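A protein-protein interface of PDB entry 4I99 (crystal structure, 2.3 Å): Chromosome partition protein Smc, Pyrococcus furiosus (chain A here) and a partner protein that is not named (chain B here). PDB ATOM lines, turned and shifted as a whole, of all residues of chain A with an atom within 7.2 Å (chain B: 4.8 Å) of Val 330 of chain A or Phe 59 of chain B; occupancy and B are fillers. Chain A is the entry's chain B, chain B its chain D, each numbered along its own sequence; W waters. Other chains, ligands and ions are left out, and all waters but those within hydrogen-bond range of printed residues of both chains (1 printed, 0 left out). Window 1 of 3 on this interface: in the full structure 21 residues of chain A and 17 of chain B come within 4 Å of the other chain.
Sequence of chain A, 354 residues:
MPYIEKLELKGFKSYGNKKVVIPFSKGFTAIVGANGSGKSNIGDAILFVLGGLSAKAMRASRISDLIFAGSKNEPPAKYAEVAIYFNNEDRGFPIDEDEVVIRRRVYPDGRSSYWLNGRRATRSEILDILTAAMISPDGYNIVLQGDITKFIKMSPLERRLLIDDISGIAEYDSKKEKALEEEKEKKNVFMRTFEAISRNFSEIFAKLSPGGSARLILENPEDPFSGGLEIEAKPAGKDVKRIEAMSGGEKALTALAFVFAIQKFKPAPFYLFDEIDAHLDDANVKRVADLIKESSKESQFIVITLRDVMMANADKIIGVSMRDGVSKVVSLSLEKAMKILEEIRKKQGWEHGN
O of Leu 332 of chain A lies within hydrogen-bond range of N of Ile 317 of chain A. The backbone carbonyl oxygen (O) of Ser 321 of chain A lies within hydrogen-bond range of the backbone NH (N) of Lys 328 of chain A (2.7 Å). The backbone NH (N) of Val 32 of chain A lies within hydrogen-bond range of the backbone carbonyl oxygen (O) of Ile 318 of chain A (3.0 Å). O of Ile 82 of chain B lies within hydrogen-bond range of N of Phe 43 of chain B, at 3.2 Å. The backbone NH of Gly 319 of chain A is in hydrogen-bond range of the backbone carbonyl oxygen of Val 330 of chain A (2.7 Å). The backbone carbonyl oxygen (O) of Val 32 of chain A sits at hydrogen-bond distance from the backbone NH (N) of Val 320 of chain A (2.9 Å).
Of the printed residues of chain B, Val 32 of chain A touches Leu 63 (3.998 Å). Of the printed residues of chain B, Met 311 of chain A touches Ala 56. Of chain B, only Phe 59, Ile 73, Gln 75 and Ile 82 come within 4 Å of Val 330 of chain A. Of the printed residues of chain B, Leu 334 of chain A touches Ile 55 (3.6 Å). Of chain A, only Ile 317 (3.6 Å), Gly 319 (3.5 Å), Val 330 (3.4 Å) and Leu 332 (3.8 Å) come within 4 Å of Phe 59 of chain B. Tyr 61 of chain B touches none of the printed residues of chain A. Printed residues of chain A within 4 Å of Leu 63 of chain B: Val 32 (3.998 Å), Gly 319 (3.3 Å), Val 320 (3.96 Å) and Ser 321 (3.7 Å). Of the printed residues of chain A, Ile 73 of chain B touches Lys 328 (3.2 Å) and Val 330 (3.6 Å). The nearest residue of chain B that does not touch Val 330 of chain A is Leu 63 of chain B (4.6 Å). The nearest residue of chain A that does not touch Phe 59 of chain B is Ile 318 of chain A (4.4 Å).
Water W1 bridges the backbone carbonyl oxygen of Val 320 of chain A (2.7 Å) and the backbone carbonyl oxygen of Leu 63 of chain B (3.4 Å).
The backbone carbonyl oxygen of Ser 331 of chain A lies within hydrogen-bond range of the side-chain amide nitrogen of Gln 75 of chain B (2.8 Å).
Of the 13 printed residues of chain B, 7 touch a printed residue of chain A. Hydrophobic or aromatic side chains of chain B within 4 Å of the printed part of chain A: Ile 55, Ala 56, Phe 59, Leu 63, Ile 73 and Ile 82. Of the 16 printed residues of chain A, 11 touch a printed residue of chain B. Among the printed residues, 16 pairs touch across the chains.
Val 32 of chain A touches Leu 63 of chain B. CE of Met 311 of chain A touches O of Ala 56 of chain B (3.3 Å). CE2 of Phe 59 of chain B touches CG2 of Ile 317 of chain A (3.6 Å). Gly 319 of chain A touches Leu 63 of chain B. Leu 63 of chain B touches Ser 321 of chain A (O to CB, 3.7 Å). CE of Lys 328 of chain A touches O of Ile 73 of chain B (3.2 Å). O of Val 330 of chain A touches CZ of Phe 59 of chain B, at 3.4 Å. Val 330 of chain A touches Gln 75 of chain B. Leu 332 of chain A touches Phe 59 of chain B (CD2 to CG, 3.8 Å). Leu 334 of chain A touches Ile 55 of chain B.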
ATOM      1  N   VAL A  21       7.530   1.175  13.859  1.00  0.00           N
ATOM      2  CA  VAL A  21       8.235   2.434  13.998  1.00  0.00           C
ATOM      3  C   VAL A  21       9.397   2.290  14.957  1.00  0.00           C
ATOM      4  O   VAL A  21       9.232   1.830  16.080  1.00  0.00           O
ATOM      5  CB  VAL A  21       7.276   3.548  14.484  1.00  0.00           C
ATOM      6  CG1 VAL A  21       8.014   4.878  14.580  1.00  0.00           C
ATOM      7  CG2 VAL A  21       6.107   3.664  13.514  1.00  0.00           C
ATOM      8  N   PRO A  23      12.283   4.490  16.768  1.00  0.00           N
ATOM      9  CA  PRO A  23      12.796   5.801  17.185  1.00  0.00           C
ATOM     10  C   PRO A  23      14.285   5.783  17.523  1.00  0.00           C
ATOM     11  O   PRO A  23      14.795   4.807  18.078  1.00  0.00           O
ATOM     12  CB  PRO A  23      11.951   6.113  18.410  1.00  0.00           C
ATOM     13  CG  PRO A  23      11.861   4.765  19.059  1.00  0.00           C
ATOM     14  CD  PRO A  23      11.592   3.824  17.888  1.00  0.00           C
ATOM     15  N   ALA A  30      21.586   1.984  21.490  1.00  0.00           N
ATOM     16  CA  ALA A  30      22.013   0.593  21.398  1.00  0.00           C
ATOM     17  C   ALA A  30      20.810  -0.249  20.966  1.00  0.00           C
ATOM     18  O   ALA A  30      19.698  -0.081  21.486  1.00  0.00           O
ATOM     19  CB  ALA A  30      22.531   0.107  22.746  1.00  0.00           C
ATOM     20  N   VAL A  32      19.515  -3.907  20.983  1.00  0.00           N
ATOM     21  CA  VAL A  32      19.807  -5.173  21.634  1.00  0.00           C
ATOM     22  C   VAL A  32      18.686  -6.182  21.455  1.00  0.00           C
ATOM     23  O   VAL A  32      17.602  -5.838  20.957  1.00  0.00           O
ATOM     24  CB  VAL A  32      20.047  -4.963  23.145  1.00  0.00           C
ATOM     25  CG1 VAL A  32      21.179  -3.962  23.364  1.00  0.00           C
ATOM     26  CG2 VAL A  32      18.760  -4.457  23.812  1.00  0.00           C
ATOM     27  N   MET A 311      25.538  -1.877  25.882  1.00  0.00           N
ATOM     28  CA  MET A 311      24.183  -1.341  25.976  1.00  0.00           C
ATOM     29  C   MET A 311      23.977  -0.474  27.204  1.00  0.00           C
ATOM     30  O   MET A 311      23.208   0.491  27.174  1.00  0.00           O
ATOM     31  CB  MET A 311      23.156  -2.465  25.962  1.00  0.00           C
ATOM     32  CG  MET A 311      23.180  -3.360  27.165  1.00  0.00           C
ATOM     33  SD  MET A 311      21.730  -4.639  27.050  1.00  0.00           S
ATOM     34  CE  MET A 311      20.264  -3.422  27.325  1.00  0.00           C
ATOM     35  N   ILE A 317      17.721   2.799  24.192  1.00  0.00           N
ATOM     36  CA  ILE A 317      17.821   1.416  23.779  1.00  0.00           C
ATOM     37  C   ILE A 317      16.637   0.947  22.951  1.00  0.00           C
ATOM     38  O   ILE A 317      15.483   1.242  23.275  1.00  0.00           O
ATOM     39  CB  ILE A 317      17.922   0.501  24.994  1.00  0.00           C
ATOM     40  CG1 ILE A 317      19.174   0.838  25.798  1.00  0.00           C
ATOM     41  CG2 ILE A 317      17.951  -0.942  24.540  1.00  0.00           C
ATOM     42  CD1 ILE A 317      19.255   0.141  27.137  1.00  0.00           C
ATOM     43  N   ILE A 318      16.929   0.215  21.879  1.00  0.00           N
ATOM     44  CA  ILE A 318      15.884  -0.338  21.028  1.00  0.00           C
ATOM     45  C   ILE A 318      15.888  -1.843  21.285  1.00  0.00           C
ATOM     46  O   ILE A 318      16.840  -2.547  20.934  1.00  0.00           O
ATOM     47  CB  ILE A 318      16.153  -0.067  19.528  1.00  0.00           C
ATOM     48  CG1 ILE A 318      16.111   1.438  19.254  1.00  0.00           C
ATOM     49  CG2 ILE A 318      15.101  -0.764  18.667  1.00  0.00           C
ATOM     50  CD1 ILE A 318      14.759   2.070  19.530  1.00  0.00           C
ATOM     51  N   GLY A 319      14.834  -2.325  21.938  1.00  0.00           N
ATOM     52  CA  GLY A 319      14.732  -3.742  22.236  1.00  0.00           C
ATOM     53  C   GLY A 319      14.069  -4.475  21.089  1.00  0.00           C
ATOM     54  O   GLY A 319      12.932  -4.178  20.726  1.00  0.00           O
ATOM     55  N   VAL A 320      14.778  -5.429  20.503  1.00  0.00           N
ATOM     56  CA  VAL A 320      14.223  -6.178  19.392  1.00  0.00           C
ATOM     57  C   VAL A 320      13.952  -7.601  19.833  1.00  0.00           C
ATOM     58  O   VAL A 320      14.807  -8.257  20.430  1.00  0.00           O
ATOM     59  CB  VAL A 320      15.196  -6.188  18.175  1.00  0.00           C
ATOM     60  CG1 VAL A 320      14.586  -6.976  17.010  1.00  0.00           C
ATOM     61  CG2 VAL A 320      15.512  -4.743  17.749  1.00  0.00           C
ATOM     62  N   SER A 321      12.744  -8.075  19.559  1.00  0.00           N
ATOM     63  CA  SER A 321      12.388  -9.436  19.918  1.00  0.00           C
ATOM     64  C   SER A 321      11.522 -10.011  18.825  1.00  0.00           C
ATOM     65  O   SER A 321      10.940  -9.285  18.027  1.00  0.00           O
ATOM     66  CB  SER A 321      11.642  -9.483  21.255  1.00  0.00           C
ATOM     67  OG  SER A 321      10.434  -8.764  21.178  1.00  0.00           O
ATOM     68  N   LYS A 328       9.721  -7.574  16.411  1.00  0.00           N
ATOM     69  CA  LYS A 328       8.992  -6.543  17.132  1.00  0.00           C
ATOM     70  C   LYS A 328      10.017  -5.644  17.845  1.00  0.00           C
ATOM     71  O   LYS A 328      11.120  -6.091  18.165  1.00  0.00           O
ATOM     72  CB  LYS A 328       8.061  -7.224  18.135  1.00  0.00           C
ATOM     73  CG  LYS A 328       7.475  -6.315  19.183  1.00  0.00           C
ATOM     74  CD  LYS A 328       6.638  -7.125  20.166  1.00  0.00           C
ATOM     75  CE  LYS A 328       6.413  -6.355  21.446  1.00  0.00           C
ATOM     76  NZ  LYS A 328       7.711  -6.117  22.144  1.00  0.00           N
ATOM     77  N   VAL A 329       9.651  -4.387  18.095  1.00  0.00           N
ATOM     78  CA  VAL A 329      10.547  -3.421  18.735  1.00  0.00           C
ATOM     79  C   VAL A 329       9.930  -2.678  19.926  1.00  0.00           C
ATOM     80  O   VAL A 329       8.722  -2.432  19.966  1.00  0.00           O
ATOM     81  CB  VAL A 329      11.012  -2.352  17.706  1.00  0.00           C
ATOM     82  CG1 VAL A 329      11.765  -1.249  18.398  1.00  0.00           C
ATOM     83  CG2 VAL A 329      11.882  -2.995  16.638  1.00  0.00           C
ATOM     84  N   VAL A 330      10.772  -2.324  20.894  1.00  0.00           N
ATOM     85  CA  VAL A 330      10.341  -1.576  22.070  1.00  0.00           C
ATOM     86  C   VAL A 330      11.414  -0.530  22.344  1.00  0.00           C
ATOM     87  O   VAL A 330      12.581  -0.864  22.511  1.00  0.00           O
ATOM     88  CB  VAL A 330      10.200  -2.473  23.322  1.00  0.00           C
ATOM     89  CG1 VAL A 330       9.729  -1.644  24.492  1.00  0.00           C
ATOM     90  CG2 VAL A 330       9.219  -3.597  23.060  1.00  0.00           C
ATOM     91  N   SER A 331      11.019   0.733  22.387  1.00  0.00           N
ATOM     92  CA  SER A 331      11.966   1.804  22.630  1.00  0.00           C
ATOM     93  C   SER A 331      11.968   2.255  24.072  1.00  0.00           C
ATOM     94  O   SER A 331      10.935   2.617  24.620  1.00  0.00           O
ATOM     95  CB  SER A 331      11.660   2.990  21.718  1.00  0.00           C
ATOM     96  OG  SER A 331      10.269   3.237  21.666  1.00  0.00           O
ATOM     97  N   LEU A 332      13.151   2.239  24.672  1.00  0.00           N
ATOM     98  CA  LEU A 332      13.339   2.641  26.056  1.00  0.00           C
ATOM     99  C   LEU A 332      14.395   3.743  26.150  1.00  0.00           C
ATOM    100  O   LEU A 332      15.492   3.618  25.601  1.00  0.00           O
ATOM    101  CB  LEU A 332      13.785   1.435  26.881  1.00  0.00           C
ATOM    102  CG  LEU A 332      14.249   1.702  28.311  1.00  0.00           C
ATOM    103  CD1 LEU A 332      13.063   2.161  29.141  1.00  0.00           C
ATOM    104  CD2 LEU A 332      14.873   0.431  28.892  1.00  0.00           C
ATOM    105  N   LEU A 334      16.798   5.588  28.612  1.00  0.00           N
ATOM    106  CA  LEU A 334      17.405   5.597  29.937  1.00  0.00           C
ATOM    107  C   LEU A 334      17.448   7.024  30.467  1.00  0.00           C
ATOM    108  O   LEU A 334      17.472   7.249  31.677  1.00  0.00           O
ATOM    109  CB  LEU A 334      18.819   5.024  29.884  1.00  0.00           C
ATOM    110  CG  LEU A 334      18.957   3.548  29.511  1.00  0.00           C
ATOM    111  CD1 LEU A 334      20.410   3.127  29.677  1.00  0.00           C
ATOM    112  CD2 LEU A 334      18.060   2.699  30.398  1.00  0.00           C
ATOM    113  N   PHE B  43       6.530  -1.994  33.518  1.00  0.00           N
ATOM    114  CA  PHE B  43       7.959  -2.291  33.485  1.00  0.00           C
ATOM    115  C   PHE B  43       8.631  -1.742  34.745  1.00  0.00           C
ATOM    116  O   PHE B  43       9.389  -2.444  35.421  1.00  0.00           O
ATOM    117  CB  PHE B  43       8.599  -1.666  32.236  1.00  0.00           C
ATOM    118  CG  PHE B  43      10.090  -1.850  32.161  1.00  0.00           C
ATOM    119  CD1 PHE B  43      10.646  -3.127  32.086  1.00  0.00           C
ATOM    120  CD2 PHE B  43      10.940  -0.747  32.188  1.00  0.00           C
ATOM    121  CE1 PHE B  43      12.025  -3.305  32.041  1.00  0.00           C
ATOM    122  CE2 PHE B  43      12.319  -0.913  32.143  1.00  0.00           C
ATOM    123  CZ  PHE B  43      12.864  -2.196  32.071  1.00  0.00           C
ATOM    124  N   ILE B  55      18.444  -1.414  34.921  1.00  0.00           N
ATOM    125  CA  ILE B  55      17.241  -1.122  34.149  1.00  0.00           C
ATOM    126  C   ILE B  55      17.392  -1.670  32.728  1.00  0.00           C
ATOM    127  O   ILE B  55      16.401  -1.971  32.060  1.00  0.00           O
ATOM    128  CB  ILE B  55      16.970   0.401  34.078  1.00  0.00           C
ATOM    129  CG1 ILE B  55      15.796   0.681  33.132  1.00  0.00           C
ATOM    130  CG2 ILE B  55      18.219   1.133  33.611  1.00  0.00           C
ATOM    131  CD1 ILE B  55      15.447   2.150  32.997  1.00  0.00           C
ATOM    132  N   ALA B  56      18.637  -1.803  32.277  1.00  0.00           N
ATOM    133  CA  ALA B  56      18.921  -2.315  30.941  1.00  0.00           C
ATOM    134  C   ALA B  56      18.881  -3.842  30.907  1.00  0.00           C
ATOM    135  O   ALA B  56      18.435  -4.434  29.925  1.00  0.00           O
ATOM    136  CB  ALA B  56      20.282  -1.809  30.461  1.00  0.00           C
ATOM    137  N   ARG B  57      19.350  -4.476  31.976  1.00  0.00           N
ATOM    138  CA  ARG B  57      19.340  -5.934  32.048  1.00  0.00           C
ATOM    139  C   ARG B  57      17.899  -6.417  32.149  1.00  0.00           C
ATOM    140  O   ARG B  57      17.498  -7.343  31.449  1.00  0.00           O
ATOM    141  CB  ARG B  57      20.141  -6.413  33.256  1.00  0.00           C
ATOM    142  N   THR B  58      17.120  -5.780  33.020  1.00  0.00           N
ATOM    143  CA  THR B  58      15.714  -6.135  33.198  1.00  0.00           C
ATOM    144  C   THR B  58      15.047  -6.122  31.829  1.00  0.00           C
ATOM    145  O   THR B  58      14.292  -7.035  31.479  1.00  0.00           O
ATOM    146  CB  THR B  58      14.985  -5.116  34.099  1.00  0.00           C
ATOM    147  OG1 THR B  58      15.689  -4.981  35.340  1.00  0.00           O
ATOM    148  CG2 THR B  58      13.557  -5.576  34.377  1.00  0.00           C
ATOM    149  N   PHE B  59      15.343  -5.075  31.064  1.00  0.00           N
ATOM    150  CA  PHE B  59      14.803  -4.903  29.720  1.00  0.00           C
ATOM    151  C   PHE B  59      15.234  -6.040  28.801  1.00  0.00           C
ATOM    152  O   PHE B  59      14.407  -6.641  28.120  1.00  0.00           O
ATOM    153  CB  PHE B  59      15.267  -3.566  29.138  1.00  0.00           C
ATOM    154  CG  PHE B  59      14.663  -3.241  27.801  1.00  0.00           C
ATOM    155  CD1 PHE B  59      13.286  -3.296  27.612  1.00  0.00           C
ATOM    156  CD2 PHE B  59      15.467  -2.847  26.738  1.00  0.00           C
ATOM    157  CE1 PHE B  59      12.719  -2.961  26.382  1.00  0.00           C
ATOM    158  CE2 PHE B  59      14.909  -2.508  25.504  1.00  0.00           C
ATOM    159  CZ  PHE B  59      13.532  -2.565  25.327  1.00  0.00           C
ATOM    160  N   LEU B  60      16.531  -6.336  28.793  1.00  0.00           N
ATOM    161  CA  LEU B  60      17.068  -7.403  27.954  1.00  0.00           C
ATOM    162  C   LEU B  60      16.400  -8.742  28.260  1.00  0.00           C
ATOM    163  O   LEU B  60      15.986  -9.459  27.347  1.00  0.00           O
ATOM    164  CB  LEU B  60      18.586  -7.524  28.155  1.00  0.00           C
ATOM    165  CG  LEU B  60      19.341  -8.598  27.356  1.00  0.00           C
ATOM    166  CD1 LEU B  60      19.205  -8.335  25.862  1.00  0.00           C
ATOM    167  CD2 LEU B  60      20.804  -8.598  27.761  1.00  0.00           C
ATOM    168  N   TYR B  61      16.297  -9.069  29.545  1.00  0.00           N
ATOM    169  CA  TYR B  61      15.686 -10.324  29.980  1.00  0.00           C
ATOM    170  C   TYR B  61      14.226 -10.451  29.541  1.00  0.00           C
ATOM    171  O   TYR B  61      13.761 -11.548  29.208  1.00  0.00           O
ATOM    172  CB  TYR B  61      15.808 -10.461  31.503  1.00  0.00           C
ATOM    173  CG  TYR B  61      17.232 -10.695  31.973  1.00  0.00           C
ATOM    174  CD1 TYR B  61      17.954 -11.806  31.531  1.00  0.00           C
ATOM    175  CD2 TYR B  61      17.863  -9.809  32.851  1.00  0.00           C
ATOM    176  CE1 TYR B  61      19.265 -12.032  31.946  1.00  0.00           C
ATOM    177  CE2 TYR B  61      19.179 -10.024  33.275  1.00  0.00           C
ATOM    178  CZ  TYR B  61      19.872 -11.139  32.817  1.00  0.00           C
ATOM    179  OH  TYR B  61      21.170 -11.372  33.222  1.00  0.00           O
ATOM    180  N   LEU B  62      13.505  -9.332  29.544  1.00  0.00           N
ATOM    181  CA  LEU B  62      12.111  -9.336  29.114  1.00  0.00           C
ATOM    182  C   LEU B  62      12.060  -9.642  27.624  1.00  0.00           C
ATOM    183  O   LEU B  62      11.216 -10.416  27.168  1.00  0.00           O
ATOM    184  CB  LEU B  62      11.446  -7.983  29.397  1.00  0.00           C
ATOM    185  CG  LEU B  62      10.852  -7.792  30.801  1.00  0.00           C
ATOM    186  CD1 LEU B  62      10.414  -6.337  30.989  1.00  0.00           C
ATOM    187  CD2 LEU B  62       9.670  -8.740  30.994  1.00  0.00           C
ATOM    188  N   LEU B  63      12.973  -9.030  26.871  1.00  0.00           N
ATOM    189  CA  LEU B  63      13.047  -9.252  25.430  1.00  0.00           C
ATOM    190  C   LEU B  63      13.325 -10.727  25.185  1.00  0.00           C
ATOM    191  O   LEU B  63      12.756 -11.333  24.276  1.00  0.00           O
ATOM    192  CB  LEU B  63      14.155  -8.398  24.812  1.00  0.00           C
ATOM    193  CG  LEU B  63      13.963  -6.883  24.909  1.00  0.00           C
ATOM    194  CD1 LEU B  63      15.197  -6.184  24.369  1.00  0.00           C
ATOM    195  CD2 LEU B  63      12.718  -6.464  24.135  1.00  0.00           C
ATOM    196  N   ILE B  73       5.442  -7.994  25.514  1.00  0.00           N
ATOM    197  CA  ILE B  73       5.696  -6.604  25.871  1.00  0.00           C
ATOM    198  C   ILE B  73       4.741  -5.665  25.144  1.00  0.00           C
ATOM    199  O   ILE B  73       4.478  -5.824  23.955  1.00  0.00           O
ATOM    200  CB  ILE B  73       7.159  -6.225  25.558  1.00  0.00           C
ATOM    201  CG1 ILE B  73       8.098  -7.194  26.288  1.00  0.00           C
ATOM    202  CG2 ILE B  73       7.432  -4.782  25.978  1.00  0.00           C
ATOM    203  CD1 ILE B  73       9.567  -7.061  25.918  1.00  0.00           C
ATOM    204  N   GLN B  75       3.710  -1.603  24.249  1.00  0.00           N
ATOM    205  CA  GLN B  75       4.121  -0.206  24.194  1.00  0.00           C
ATOM    206  C   GLN B  75       3.331   0.447  23.066  1.00  0.00           C
ATOM    207  O   GLN B  75       3.510   0.111  21.896  1.00  0.00           O
ATOM    208  CB  GLN B  75       5.626  -0.080  23.943  1.00  0.00           C
ATOM    209  CG  GLN B  75       6.125   1.359  24.030  1.00  0.00           C
ATOM    210  CD  GLN B  75       7.631   1.463  23.951  1.00  0.00           C
ATOM    211  OE1 GLN B  75       8.246   0.996  22.997  1.00  0.00           O
ATOM    212  NE2 GLN B  75       8.232   2.083  24.955  1.00  0.00           N
ATOM    213  N   ILE B  82       5.875   0.929  28.914  1.00  0.00           N
ATOM    214  CA  ILE B  82       6.036  -0.489  28.631  1.00  0.00           C
ATOM    215  C   ILE B  82       5.219  -1.291  29.637  1.00  0.00           C
ATOM    216  O   ILE B  82       5.208  -0.975  30.827  1.00  0.00           O
ATOM    217  CB  ILE B  82       7.527  -0.912  28.731  1.00  0.00           C
ATOM    218  CG1 ILE B  82       8.356  -0.132  27.710  1.00  0.00           C
ATOM    219  CG2 ILE B  82       7.672  -2.411  28.487  1.00  0.00           C
ATOM    220  CD1 ILE B  82       9.823  -0.481  27.725  1.00  0.00           C
HETATM  221  O   HOH W   1      15.137 -10.402  22.093  1.00  0.00           O
